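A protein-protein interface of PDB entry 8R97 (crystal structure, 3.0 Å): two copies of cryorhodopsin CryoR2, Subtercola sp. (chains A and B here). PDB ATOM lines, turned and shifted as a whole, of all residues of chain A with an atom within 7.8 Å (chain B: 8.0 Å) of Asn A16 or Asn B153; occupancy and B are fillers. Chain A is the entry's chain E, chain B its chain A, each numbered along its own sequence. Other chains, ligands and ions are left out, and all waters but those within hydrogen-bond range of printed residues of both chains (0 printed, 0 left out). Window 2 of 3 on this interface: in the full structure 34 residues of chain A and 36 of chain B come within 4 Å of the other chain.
O of Phe B145 is in hydrogen-bond range of N of Val B150, at 3.0 Å. O of Leu B146 lies within hydrogen-bond range of N of Ile B151, 2.6 Å away. The backbone carbonyl oxygen (O) of Ile B149 sits at hydrogen-bond distance from the backbone NH (N) of Gly B154 (3.5 Å). The side-chain amide oxygen of Asn A16 sits at hydrogen-bond distance from the indole nitrogen of Trp A87.
Asn B153 touches Asn A16 (ND2 to ND2, 3.6 Å). CB of Ala A17 touches O of Val B150 (3.4 Å). Gln A20 touches Asn B95 (NE2 to OD1, 3.97 Å). Gln A20 touches Phe B145. Gln A20 touches Ile B149. CD2 of Leu A21 touches CD2 of Leu B146, 3.9 Å away. Val B150 touches Leu A21. Asp B91 touches Ser A82 (OD2 to OG, 3.7 Å).
Ser A15 touches none of the printed residues of chain B. Of chain B, only Val B150 (3.4 Å) comes within 4 Å of Ala A17. Of the printed residues of chain B, Leu A21 touches Leu B146 and Val B150. Of the printed residues of chain A, Phe B145 touches Gln A20 (3.5 Å). Printed residues of chain A within 4 Å of Leu B146: Leu A21 (3.9 Å). Printed residues of chain A within 4 Å of Ile B149: Gln A20. Printed residues of chain A within 4 Å of Val B150: Ala A17 (3.4 Å) and Leu A21 (3.7 Å). Of the printed residues of chain A, Asn B153 touches Asn A16. The nearest residue of chain B that does not touch Asn A16 is Val B150 (5.6 Å). The nearest printed residue of chain A that does not touch Ile B149 is Ala A17 (5.7 Å).
Of the 19 printed residues of chain B, 7 touch a printed residue of chain A. Printed residues of chain A that touch a printed residue of chain B: Asn A16, Ala A17, Gln A20, Leu A21 and Ser A82. Hydrophobic or aromatic side chains of chain A within 4 Å of the printed part of chain B: Ala A17 and Leu A21. Among the printed residues, 8 pairs touch across the chains. Among the printed residues, no Asp or Glu carboxylate lies within 4 Å of a Lys or Arg side-chain nitrogen of the other chain.
No position is printed for both chains.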
ATOM      1  N   THR A  13     -12.879  25.773  -0.973  1.00  0.00           N
ATOM      2  CA  THR A  13     -13.940  24.732  -0.941  1.00  0.00           C
ATOM      3  C   THR A  13     -13.729  23.867   0.306  1.00  0.00           C
ATOM      4  O   THR A  13     -12.558  23.595   0.640  1.00  0.00           O
ATOM      5  CB  THR A  13     -13.935  23.899  -2.231  1.00  0.00           C
ATOM      6  OG1 THR A  13     -14.298  24.764  -3.307  1.00  0.00           O
ATOM      7  CG2 THR A  13     -14.880  22.719  -2.181  1.00  0.00           C
ATOM      8  N   LEU A  14     -14.817  23.448   0.960  1.00  0.00           N
ATOM      9  CA  LEU A  14     -14.776  22.673   2.230  1.00  0.00           C
ATOM     10  C   LEU A  14     -15.255  21.234   2.010  1.00  0.00           C
ATOM     11  O   LEU A  14     -16.173  21.021   1.188  1.00  0.00           O
ATOM     12  CB  LEU A  14     -15.652  23.381   3.268  1.00  0.00           C
ATOM     13  CG  LEU A  14     -15.222  24.797   3.641  1.00  0.00           C
ATOM     14  CD1 LEU A  14     -16.183  25.397   4.655  1.00  0.00           C
ATOM     15  CD2 LEU A  14     -13.798  24.826   4.177  1.00  0.00           C
ATOM     16  N   SER A  15     -14.643  20.289   2.730  1.00  0.00           N
ATOM     17  CA  SER A  15     -15.014  18.852   2.743  1.00  0.00           C
ATOM     18  C   SER A  15     -16.311  18.704   3.539  1.00  0.00           C
ATOM     19  O   SER A  15     -16.648  19.646   4.285  1.00  0.00           O
ATOM     20  CB  SER A  15     -13.914  18.004   3.327  1.00  0.00           C
ATOM     21  OG  SER A  15     -13.815  18.201   4.728  1.00  0.00           O
ATOM     22  N   ASN A  16     -17.010  17.575   3.382  1.00  0.00           N
ATOM     23  CA  ASN A  16     -18.268  17.283   4.120  1.00  0.00           C
ATOM     24  C   ASN A  16     -17.953  17.261   5.620  1.00  0.00           C
ATOM     25  O   ASN A  16     -18.771  17.780   6.404  1.00  0.00           O
ATOM     26  CB  ASN A  16     -18.918  15.983   3.641  1.00  0.00           C
ATOM     27  CG  ASN A  16     -19.501  16.102   2.249  1.00  0.00           C
ATOM     28  OD1 ASN A  16     -19.463  17.170   1.643  1.00  0.00           O
ATOM     29  ND2 ASN A  16     -20.042  15.010   1.734  1.00  0.00           N
ATOM     30  N   ALA A  17     -16.799  16.699   5.991  1.00  0.00           N
ATOM     31  CA  ALA A  17     -16.306  16.608   7.385  1.00  0.00           C
ATOM     32  C   ALA A  17     -16.072  18.019   7.936  1.00  0.00           C
ATOM     33  O   ALA A  17     -16.574  18.317   9.037  1.00  0.00           O
ATOM     34  CB  ALA A  17     -15.047  15.781   7.435  1.00  0.00           C
ATOM     35  N   GLU A  18     -15.336  18.849   7.191  1.00  0.00           N
ATOM     36  CA  GLU A  18     -15.022  20.254   7.565  1.00  0.00           C
ATOM     37  C   GLU A  18     -16.335  21.013   7.790  1.00  0.00           C
ATOM     38  O   GLU A  18     -16.480  21.639   8.863  1.00  0.00           O
ATOM     39  CB  GLU A  18     -14.158  20.906   6.482  1.00  0.00           C
ATOM     40  CG  GLU A  18     -12.736  20.368   6.435  1.00  0.00           C
ATOM     41  CD  GLU A  18     -11.893  20.848   5.263  1.00  0.00           C
ATOM     42  OE1 GLU A  18     -10.682  20.547   5.245  1.00  0.00           O
ATOM     43  OE2 GLU A  18     -12.448  21.517   4.365  1.00  0.00           O
ATOM     44  N   HIS A  19     -17.259  20.932   6.826  1.00  0.00           N
ATOM     45  CA  HIS A  19     -18.586  21.607   6.851  1.00  0.00           C
ATOM     46  C   HIS A  19     -19.333  21.220   8.133  1.00  0.00           C
ATOM     47  O   HIS A  19     -19.940  22.115   8.755  1.00  0.00           O
ATOM     48  CB  HIS A  19     -19.394  21.260   5.593  1.00  0.00           C
ATOM     49  CG  HIS A  19     -20.563  22.160   5.358  1.00  0.00           C
ATOM     50  ND1 HIS A  19     -21.834  21.860   5.817  1.00  0.00           N
ATOM     51  CD2 HIS A  19     -20.661  23.345   4.715  1.00  0.00           C
ATOM     52  CE1 HIS A  19     -22.663  22.826   5.468  1.00  0.00           C
ATOM     53  NE2 HIS A  19     -21.967  23.749   4.788  1.00  0.00           N
ATOM     54  N   GLN A  20     -19.276  19.939   8.509  1.00  0.00           N
ATOM     55  CA  GLN A  20     -19.981  19.377   9.693  1.00  0.00           C
ATOM     56  C   GLN A  20     -19.355  19.944  10.974  1.00  0.00           C
ATOM     57  O   GLN A  20     -20.115  20.353  11.874  1.00  0.00           O
ATOM     58  CB  GLN A  20     -19.904  17.849   9.686  1.00  0.00           C
ATOM     59  CG  GLN A  20     -21.082  17.173  10.373  1.00  0.00           C
ATOM     60  CD  GLN A  20     -22.290  17.068   9.473  1.00  0.00           C
ATOM     61  OE1 GLN A  20     -22.219  17.308   8.271  1.00  0.00           O
ATOM     62  NE2 GLN A  20     -23.415  16.682  10.051  1.00  0.00           N
ATOM     63  N   LEU A  21     -18.019  19.964  11.048  1.00  0.00           N
ATOM     64  CA  LEU A  21     -17.249  20.453  12.225  1.00  0.00           C
ATOM     65  C   LEU A  21     -17.571  21.928  12.483  1.00  0.00           C
ATOM     66  O   LEU A  21     -17.873  22.268  13.642  1.00  0.00           O
ATOM     67  CB  LEU A  21     -15.752  20.247  11.978  1.00  0.00           C
ATOM     68  CG  LEU A  21     -15.247  18.819  12.186  1.00  0.00           C
ATOM     69  CD1 LEU A  21     -13.789  18.692  11.774  1.00  0.00           C
ATOM     70  CD2 LEU A  21     -15.426  18.383  13.633  1.00  0.00           C
ATOM     71  N   ILE A  22     -17.514  22.763  11.443  1.00  0.00           N
ATOM     72  CA  ILE A  22     -17.779  24.230  11.541  1.00  0.00           C
ATOM     73  C   ILE A  22     -19.186  24.440  12.109  1.00  0.00           C
ATOM     74  O   ILE A  22     -19.320  25.208  13.080  1.00  0.00           O
ATOM     75  CB  ILE A  22     -17.595  24.918  10.174  1.00  0.00           C
ATOM     76  CG1 ILE A  22     -16.204  24.648   9.594  1.00  0.00           C
ATOM     77  CG2 ILE A  22     -17.885  26.408  10.283  1.00  0.00           C
ATOM     78  CD1 ILE A  22     -16.006  25.182   8.195  1.00  0.00           C
ATOM     79  N   PHE A  76     -23.646  30.786   6.989  1.00  0.00           N
ATOM     80  CA  PHE A  76     -22.898  29.524   6.751  1.00  0.00           C
ATOM     81  C   PHE A  76     -23.749  28.561   5.917  1.00  0.00           C
ATOM     82  O   PHE A  76     -23.211  27.914   4.995  1.00  0.00           O
ATOM     83  CB  PHE A  76     -22.494  28.888   8.084  1.00  0.00           C
ATOM     84  CG  PHE A  76     -21.856  27.528   7.965  1.00  0.00           C
ATOM     85  CD1 PHE A  76     -22.597  26.376   8.181  1.00  0.00           C
ATOM     86  CD2 PHE A  76     -20.517  27.397   7.634  1.00  0.00           C
ATOM     87  CE1 PHE A  76     -22.009  25.125   8.077  1.00  0.00           C
ATOM     88  CE2 PHE A  76     -19.933  26.145   7.524  1.00  0.00           C
ATOM     89  CZ  PHE A  76     -20.680  25.011   7.743  1.00  0.00           C
ATOM     90  N   ASP A  81     -22.573  25.591  -1.199  1.00  0.00           N
ATOM     91  CA  ASP A  81     -23.439  24.683  -1.998  1.00  0.00           C
ATOM     92  C   ASP A  81     -22.757  23.312  -2.055  1.00  0.00           C
ATOM     93  O   ASP A  81     -21.530  23.281  -2.294  1.00  0.00           O
ATOM     94  CB  ASP A  81     -23.674  25.252  -3.399  1.00  0.00           C
ATOM     95  CG  ASP A  81     -24.157  26.692  -3.398  1.00  0.00           C
ATOM     96  OD1 ASP A  81     -25.229  26.949  -2.821  1.00  0.00           O
ATOM     97  OD2 ASP A  81     -23.454  27.547  -3.972  1.00  0.00           O
ATOM     98  N   SER A  82     -23.513  22.231  -1.828  1.00  0.00           N
ATOM     99  CA  SER A  82     -23.014  20.830  -1.836  1.00  0.00           C
ATOM    100  C   SER A  82     -22.884  20.345  -3.282  1.00  0.00           C
ATOM    101  O   SER A  82     -23.884  20.419  -4.020  1.00  0.00           O
ATOM    102  CB  SER A  82     -23.907  19.919  -1.040  1.00  0.00           C
ATOM    103  OG  SER A  82     -23.317  18.635  -0.898  1.00  0.00           O
ATOM    104  N   THR A  83     -21.693  19.874  -3.664  1.00  0.00           N
ATOM    105  CA  THR A  83     -21.357  19.406  -5.034  1.00  0.00           C
ATOM    106  C   THR A  83     -20.651  18.051  -4.942  1.00  0.00           C
ATOM    107  O   THR A  83     -20.669  17.443  -3.850  1.00  0.00           O
ATOM    108  CB  THR A  83     -20.479  20.429  -5.771  1.00  0.00           C
ATOM    109  OG1 THR A  83     -19.248  20.544  -5.056  1.00  0.00           O
ATOM    110  CG2 THR A  83     -21.135  21.787  -5.902  1.00  0.00           C
ATOM    111  N   ALA A  84     -20.064  17.603  -6.054  1.00  0.00           N
ATOM    112  CA  ALA A  84     -19.285  16.350  -6.160  1.00  0.00           C
ATOM    113  C   ALA A  84     -17.895  16.574  -5.552  1.00  0.00           C
ATOM    114  O   ALA A  84     -17.240  15.577  -5.197  1.00  0.00           O
ATOM    115  CB  ALA A  84     -19.202  15.920  -7.604  1.00  0.00           C
ATOM    116  N   GLY A  85     -17.480  17.840  -5.427  1.00  0.00           N
ATOM    117  CA  GLY A  85     -16.145  18.235  -4.934  1.00  0.00           C
ATOM    118  C   GLY A  85     -16.150  18.585  -3.456  1.00  0.00           C
ATOM    119  O   GLY A  85     -15.055  18.836  -2.913  1.00  0.00           O
ATOM    120  N   GLY A  86     -17.331  18.586  -2.828  1.00  0.00           N
ATOM    121  CA  GLY A  86     -17.516  18.934  -1.403  1.00  0.00           C
ATOM    122  C   GLY A  86     -18.544  20.040  -1.231  1.00  0.00           C
ATOM    123  O   GLY A  86     -19.676  19.861  -1.722  1.00  0.00           O
ATOM    124  N   TRP A  87     -18.163  21.142  -0.577  1.00  0.00           N
ATOM    125  CA  TRP A  87     -19.015  22.346  -0.376  1.00  0.00           C
ATOM    126  C   TRP A  87     -18.344  23.561  -1.024  1.00  0.00           C
ATOM    127  O   TRP A  87     -17.392  24.090  -0.424  1.00  0.00           O
ATOM    128  CB  TRP A  87     -19.283  22.581   1.113  1.00  0.00           C
ATOM    129  CG  TRP A  87     -20.178  21.553   1.729  1.00  0.00           C
ATOM    130  CD1 TRP A  87     -19.810  20.345   2.246  1.00  0.00           C
ATOM    131  CD2 TRP A  87     -21.604  21.641   1.890  1.00  0.00           C
ATOM    132  NE1 TRP A  87     -20.906  19.676   2.722  1.00  0.00           N
ATOM    133  CE2 TRP A  87     -22.021  20.448   2.517  1.00  0.00           C
ATOM    134  CE3 TRP A  87     -22.565  22.607   1.569  1.00  0.00           C
ATOM    135  CZ2 TRP A  87     -23.358  20.201   2.827  1.00  0.00           C
ATOM    136  CZ3 TRP A  87     -23.884  22.362   1.877  1.00  0.00           C
ATOM    137  CH2 TRP A  87     -24.272  21.175   2.497  1.00  0.00           C
ATOM    138  N   VAL B   6     -20.606  -0.532   8.809  1.00  0.00           N
ATOM    139  CA  VAL B   6     -21.451   0.620   9.251  1.00  0.00           C
ATOM    140  C   VAL B   6     -22.449   0.980   8.148  1.00  0.00           C
ATOM    141  O   VAL B   6     -22.009   1.308   7.036  1.00  0.00           O
ATOM    142  CB  VAL B   6     -20.603   1.850   9.626  1.00  0.00           C
ATOM    143  CG1 VAL B   6     -21.470   2.969  10.182  1.00  0.00           C
ATOM    144  CG2 VAL B   6     -19.486   1.498  10.594  1.00  0.00           C
ATOM    145  N   VAL B   8     -25.046   3.716   7.625  1.00  0.00           N
ATOM    146  CA  VAL B   8     -25.517   5.067   8.057  1.00  0.00           C
ATOM    147  C   VAL B   8     -27.043   5.071   8.081  1.00  0.00           C
ATOM    148  O   VAL B   8     -27.687   4.659   7.118  1.00  0.00           O
ATOM    149  CB  VAL B   8     -24.963   6.191   7.161  1.00  0.00           C
ATOM    150  CG1 VAL B   8     -23.448   6.265   7.227  1.00  0.00           C
ATOM    151  CG2 VAL B   8     -25.427   6.058   5.720  1.00  0.00           C
ATOM    152  N   PRO B   9     -27.659   5.536   9.192  1.00  0.00           N
ATOM    153  CA  PRO B   9     -29.116   5.539   9.331  1.00  0.00           C
ATOM    154  C   PRO B   9     -29.830   6.548   8.417  1.00  0.00           C
ATOM    155  O   PRO B   9     -30.994   6.338   8.117  1.00  0.00           O
ATOM    156  CB  PRO B   9     -29.348   5.923  10.804  1.00  0.00           C
ATOM    157  CG  PRO B   9     -27.991   5.768  11.475  1.00  0.00           C
ATOM    158  CD  PRO B   9     -26.980   6.055  10.386  1.00  0.00           C
ATOM    159  N   TRP B  10     -29.127   7.607   8.000  1.00  0.00           N
ATOM    160  CA  TRP B  10     -29.672   8.698   7.145  1.00  0.00           C
ATOM    161  C   TRP B  10     -29.693   8.260   5.673  1.00  0.00           C
ATOM    162  O   TRP B  10     -30.003   9.105   4.812  1.00  0.00           O
ATOM    163  CB  TRP B  10     -28.880   9.998   7.345  1.00  0.00           C
ATOM    164  CG  TRP B  10     -27.398   9.864   7.174  1.00  0.00           C
ATOM    165  CD1 TRP B  10     -26.698   9.860   6.004  1.00  0.00           C
ATOM    166  CD2 TRP B  10     -26.420   9.737   8.222  1.00  0.00           C
ATOM    167  NE1 TRP B  10     -25.357   9.726   6.249  1.00  0.00           N
ATOM    168  CE2 TRP B  10     -25.155   9.649   7.602  1.00  0.00           C
ATOM    169  CE3 TRP B  10     -26.489   9.680   9.619  1.00  0.00           C
ATOM    170  CZ2 TRP B  10     -23.975   9.508   8.332  1.00  0.00           C
ATOM    171  CZ3 TRP B  10     -25.322   9.542  10.340  1.00  0.00           C
ATOM    172  CH2 TRP B  10     -24.084   9.456   9.703  1.00  0.00           C
ATOM    173  N   ASP B  91     -29.256  14.990   1.008  1.00  0.00           N
ATOM    174  CA  ASP B  91     -27.890  15.288   1.517  1.00  0.00           C
ATOM    175  C   ASP B  91     -27.957  15.825   2.951  1.00  0.00           C
ATOM    176  O   ASP B  91     -26.975  15.635   3.693  1.00  0.00           O
ATOM    177  CB  ASP B  91     -27.177  16.306   0.625  1.00  0.00           C
ATOM    178  CG  ASP B  91     -26.996  15.844  -0.808  1.00  0.00           C
ATOM    179  OD1 ASP B  91     -27.663  14.863  -1.198  1.00  0.00           O
ATOM    180  OD2 ASP B  91     -26.187  16.467  -1.519  1.00  0.00           O
ATOM    181  N   ILE B  94     -28.418  13.761   7.185  1.00  0.00           N
ATOM    182  CA  ILE B  94     -27.323  13.526   8.174  1.00  0.00           C
ATOM    183  C   ILE B  94     -27.417  14.571   9.294  1.00  0.00           C
ATOM    184  O   ILE B  94     -27.116  14.216  10.455  1.00  0.00           O
ATOM    185  CB  ILE B  94     -25.943  13.549   7.484  1.00  0.00           C
ATOM    186  CG1 ILE B  94     -24.819  13.212   8.467  1.00  0.00           C
ATOM    187  CG2 ILE B  94     -25.701  14.884   6.792  1.00  0.00           C
ATOM    188  CD1 ILE B  94     -23.445  13.167   7.837  1.00  0.00           C
ATOM    189  N   ASN B  95     -27.830  15.799   8.958  1.00  0.00           N
ATOM    190  CA  ASN B  95     -27.915  16.949   9.900  1.00  0.00           C
ATOM    191  C   ASN B  95     -28.808  16.603  11.096  1.00  0.00           C
ATOM    192  O   ASN B  95     -28.524  17.108  12.203  1.00  0.00           O
ATOM    193  CB  ASN B  95     -28.401  18.220   9.199  1.00  0.00           C
ATOM    194  CG  ASN B  95     -27.330  18.828   8.322  1.00  0.00           C
ATOM    195  OD1 ASN B  95     -26.415  18.127   7.892  1.00  0.00           O
ATOM    196  ND2 ASN B  95     -27.418  20.126   8.078  1.00  0.00           N
ATOM    197  N   PHE B 145     -19.338  12.150  17.871  1.00  0.00           N
ATOM    198  CA  PHE B 145     -19.626  12.988  16.677  1.00  0.00           C
ATOM    199  C   PHE B 145     -18.579  12.703  15.593  1.00  0.00           C
ATOM    200  O   PHE B 145     -18.963  12.499  14.419  1.00  0.00           O
ATOM    201  CB  PHE B 145     -19.640  14.471  17.059  1.00  0.00           C
ATOM    202  CG  PHE B 145     -19.910  15.419  15.918  1.00  0.00           C
ATOM    203  CD1 PHE B 145     -19.011  16.424  15.597  1.00  0.00           C
ATOM    204  CD2 PHE B 145     -21.061  15.295  15.155  1.00  0.00           C
ATOM    205  CE1 PHE B 145     -19.267  17.294  14.550  1.00  0.00           C
ATOM    206  CE2 PHE B 145     -21.311  16.160  14.100  1.00  0.00           C
ATOM    207  CZ  PHE B 145     -20.416  17.162  13.804  1.00  0.00           C
ATOM    208  N   LEU B 146     -17.300  12.682  15.985  1.00  0.00           N
ATOM    209  CA  LEU B 146     -16.144  12.444  15.077  1.00  0.00           C
ATOM    210  C   LEU B 146     -16.301  11.078  14.398  1.00  0.00           C
ATOM    211  O   LEU B 146     -16.188  11.023  13.161  1.00  0.00           O
ATOM    212  CB  LEU B 146     -14.834  12.515  15.871  1.00  0.00           C
ATOM    213  CG  LEU B 146     -14.401  13.908  16.330  1.00  0.00           C
ATOM    214  CD1 LEU B 146     -13.028  13.866  16.985  1.00  0.00           C
ATOM    215  CD2 LEU B 146     -14.385  14.901  15.176  1.00  0.00           C
ATOM    216  N   GLY B 147     -16.563  10.027  15.181  1.00  0.00           N
ATOM    217  CA  GLY B 147     -16.660   8.635  14.698  1.00  0.00           C
ATOM    218  C   GLY B 147     -17.874   8.387  13.816  1.00  0.00           C
ATOM    219  O   GLY B 147     -17.705   7.778  12.742  1.00  0.00           O
ATOM    220  N   ALA B 148     -19.054   8.844  14.243  1.00  0.00           N
ATOM    221  CA  ALA B 148     -20.363   8.562  13.607  1.00  0.00           C
ATOM    222  C   ALA B 148     -20.643   9.486  12.412  1.00  0.00           C
ATOM    223  O   ALA B 148     -21.257   9.000  11.438  1.00  0.00           O
ATOM    224  CB  ALA B 148     -21.455   8.685  14.640  1.00  0.00           C
ATOM    225  N   ILE B 149     -20.231  10.758  12.476  1.00  0.00           N
ATOM    226  CA  ILE B 149     -20.595  11.782  11.450  1.00  0.00           C
ATOM    227  C   ILE B 149     -19.355  12.312  10.718  1.00  0.00           C
ATOM    228  O   ILE B 149     -19.321  12.219   9.476  1.00  0.00           O
ATOM    229  CB  ILE B 149     -21.388  12.940  12.094  1.00  0.00           C
ATOM    230  CG1 ILE B 149     -22.549  12.436  12.956  1.00  0.00           C
ATOM    231  CG2 ILE B 149     -21.863  13.915  11.025  1.00  0.00           C
ATOM    232  CD1 ILE B 149     -23.757  11.992  12.166  1.00  0.00           C
ATOM    233  N   VAL B 150     -18.393  12.879  11.449  1.00  0.00           N
ATOM    234  CA  VAL B 150     -17.237  13.625  10.866  1.00  0.00           C
ATOM    235  C   VAL B 150     -16.356  12.698  10.017  1.00  0.00           C
ATOM    236  O   VAL B 150     -16.255  12.934   8.796  1.00  0.00           O
ATOM    237  CB  VAL B 150     -16.426  14.327  11.971  1.00  0.00           C
ATOM    238  CG1 VAL B 150     -15.174  15.002  11.420  1.00  0.00           C
ATOM    239  CG2 VAL B 150     -17.290  15.323  12.737  1.00  0.00           C
ATOM    240  N   ILE B 151     -15.747  11.684  10.636  1.00  0.00           N
ATOM    241  CA  ILE B 151     -14.714  10.812   9.999  1.00  0.00           C
ATOM    242  C   ILE B 151     -15.332   9.956   8.888  1.00  0.00           C
ATOM    243  O   ILE B 151     -16.234   9.137   9.181  1.00  0.00           O
ATOM    244  CB  ILE B 151     -13.998   9.960  11.062  1.00  0.00           C
ATOM    245  CG1 ILE B 151     -13.305  10.852  12.096  1.00  0.00           C
ATOM    246  CG2 ILE B 151     -13.031   8.989  10.405  1.00  0.00           C
ATOM    247  CD1 ILE B 151     -12.424  10.113  13.063  1.00  0.00           C
ATOM    248  N   ASP B 152     -14.831  10.151   7.662  1.00  0.00           N
ATOM    249  CA  ASP B 152     -15.203   9.384   6.445  1.00  0.00           C
ATOM    250  C   ASP B 152     -16.728   9.332   6.301  1.00  0.00           C
ATOM    251  O   ASP B 152     -17.251   8.309   5.814  1.00  0.00           O
ATOM    252  CB  ASP B 152     -14.557   8.000   6.478  1.00  0.00           C
ATOM    253  CG  ASP B 152     -13.049   8.059   6.302  1.00  0.00           C
ATOM    254  OD1 ASP B 152     -12.559   9.103   5.820  1.00  0.00           O
ATOM    255  OD2 ASP B 152     -12.373   7.061   6.643  1.00  0.00           O
ATOM    256  N   ASN B 153     -17.399  10.411   6.712  1.00  0.00           N
ATOM    257  CA  ASN B 153     -18.861  10.603   6.545  1.00  0.00           C
ATOM    258  C   ASN B 153     -19.612   9.492   7.283  1.00  0.00           C
ATOM    259  O   ASN B 153     -20.738   9.162   6.852  1.00  0.00           O
ATOM    260  CB  ASN B 153     -19.191  10.684   5.055  1.00  0.00           C
ATOM    261  CG  ASN B 153     -18.410  11.787   4.371  1.00  0.00           C
ATOM    262  OD1 ASN B 153     -17.653  12.516   5.010  1.00  0.00           O
ATOM    263  ND2 ASN B 153     -18.601  11.935   3.072  1.00  0.00           N
ATOM    264  N   GLY B 154     -19.011   8.951   8.351  1.00  0.00           N
ATOM    265  CA  GLY B 154     -19.615   7.927   9.227  1.00  0.00           C
ATOM    266  C   GLY B 154     -19.753   6.576   8.544  1.00  0.00           C
ATOM    267  O   GLY B 154     -20.622   5.796   8.969  1.00  0.00           O
ATOM    268  N   THR B 155     -18.924   6.301   7.533  1.00  0.00           N
ATOM    269  CA  THR B 155     -18.922   5.030   6.759  1.00  0.00           C
ATOM    270  C   THR B 155     -17.775   4.125   7.239  1.00  0.00           C
ATOM    271  O   THR B 155     -17.747   2.950   6.832  1.00  0.00           O
ATOM    272  CB  THR B 155     -18.840   5.313   5.253  1.00  0.00           C
ATOM    273  OG1 THR B 155     -17.647   6.062   5.024  1.00  0.00           O
ATOM    274  CG2 THR B 155     -20.045   6.064   4.730  1.00  0.00           C
ATOM    275  N   ASN B 156     -16.870   4.644   8.074  1.00  0.00           N
ATOM    276  CA  ASN B 156     -15.687   3.896   8.578  1.00  0.00           C
ATOM    277  C   ASN B 156     -16.061   3.126   9.847  1.00  0.00           C
ATOM    278  O   ASN B 156     -16.232   3.777  10.899  1.00  0.00           O
ATOM    279  CB  ASN B 156     -14.500   4.821   8.854  1.00  0.00           C
ATOM    280  CG  ASN B 156     -13.267   4.061   9.294  1.00  0.00           C
ATOM    281  OD1 ASN B 156     -13.369   2.939   9.783  1.00  0.00           O
ATOM    282  ND2 ASN B 156     -12.101   4.660   9.126  1.00  0.00           N
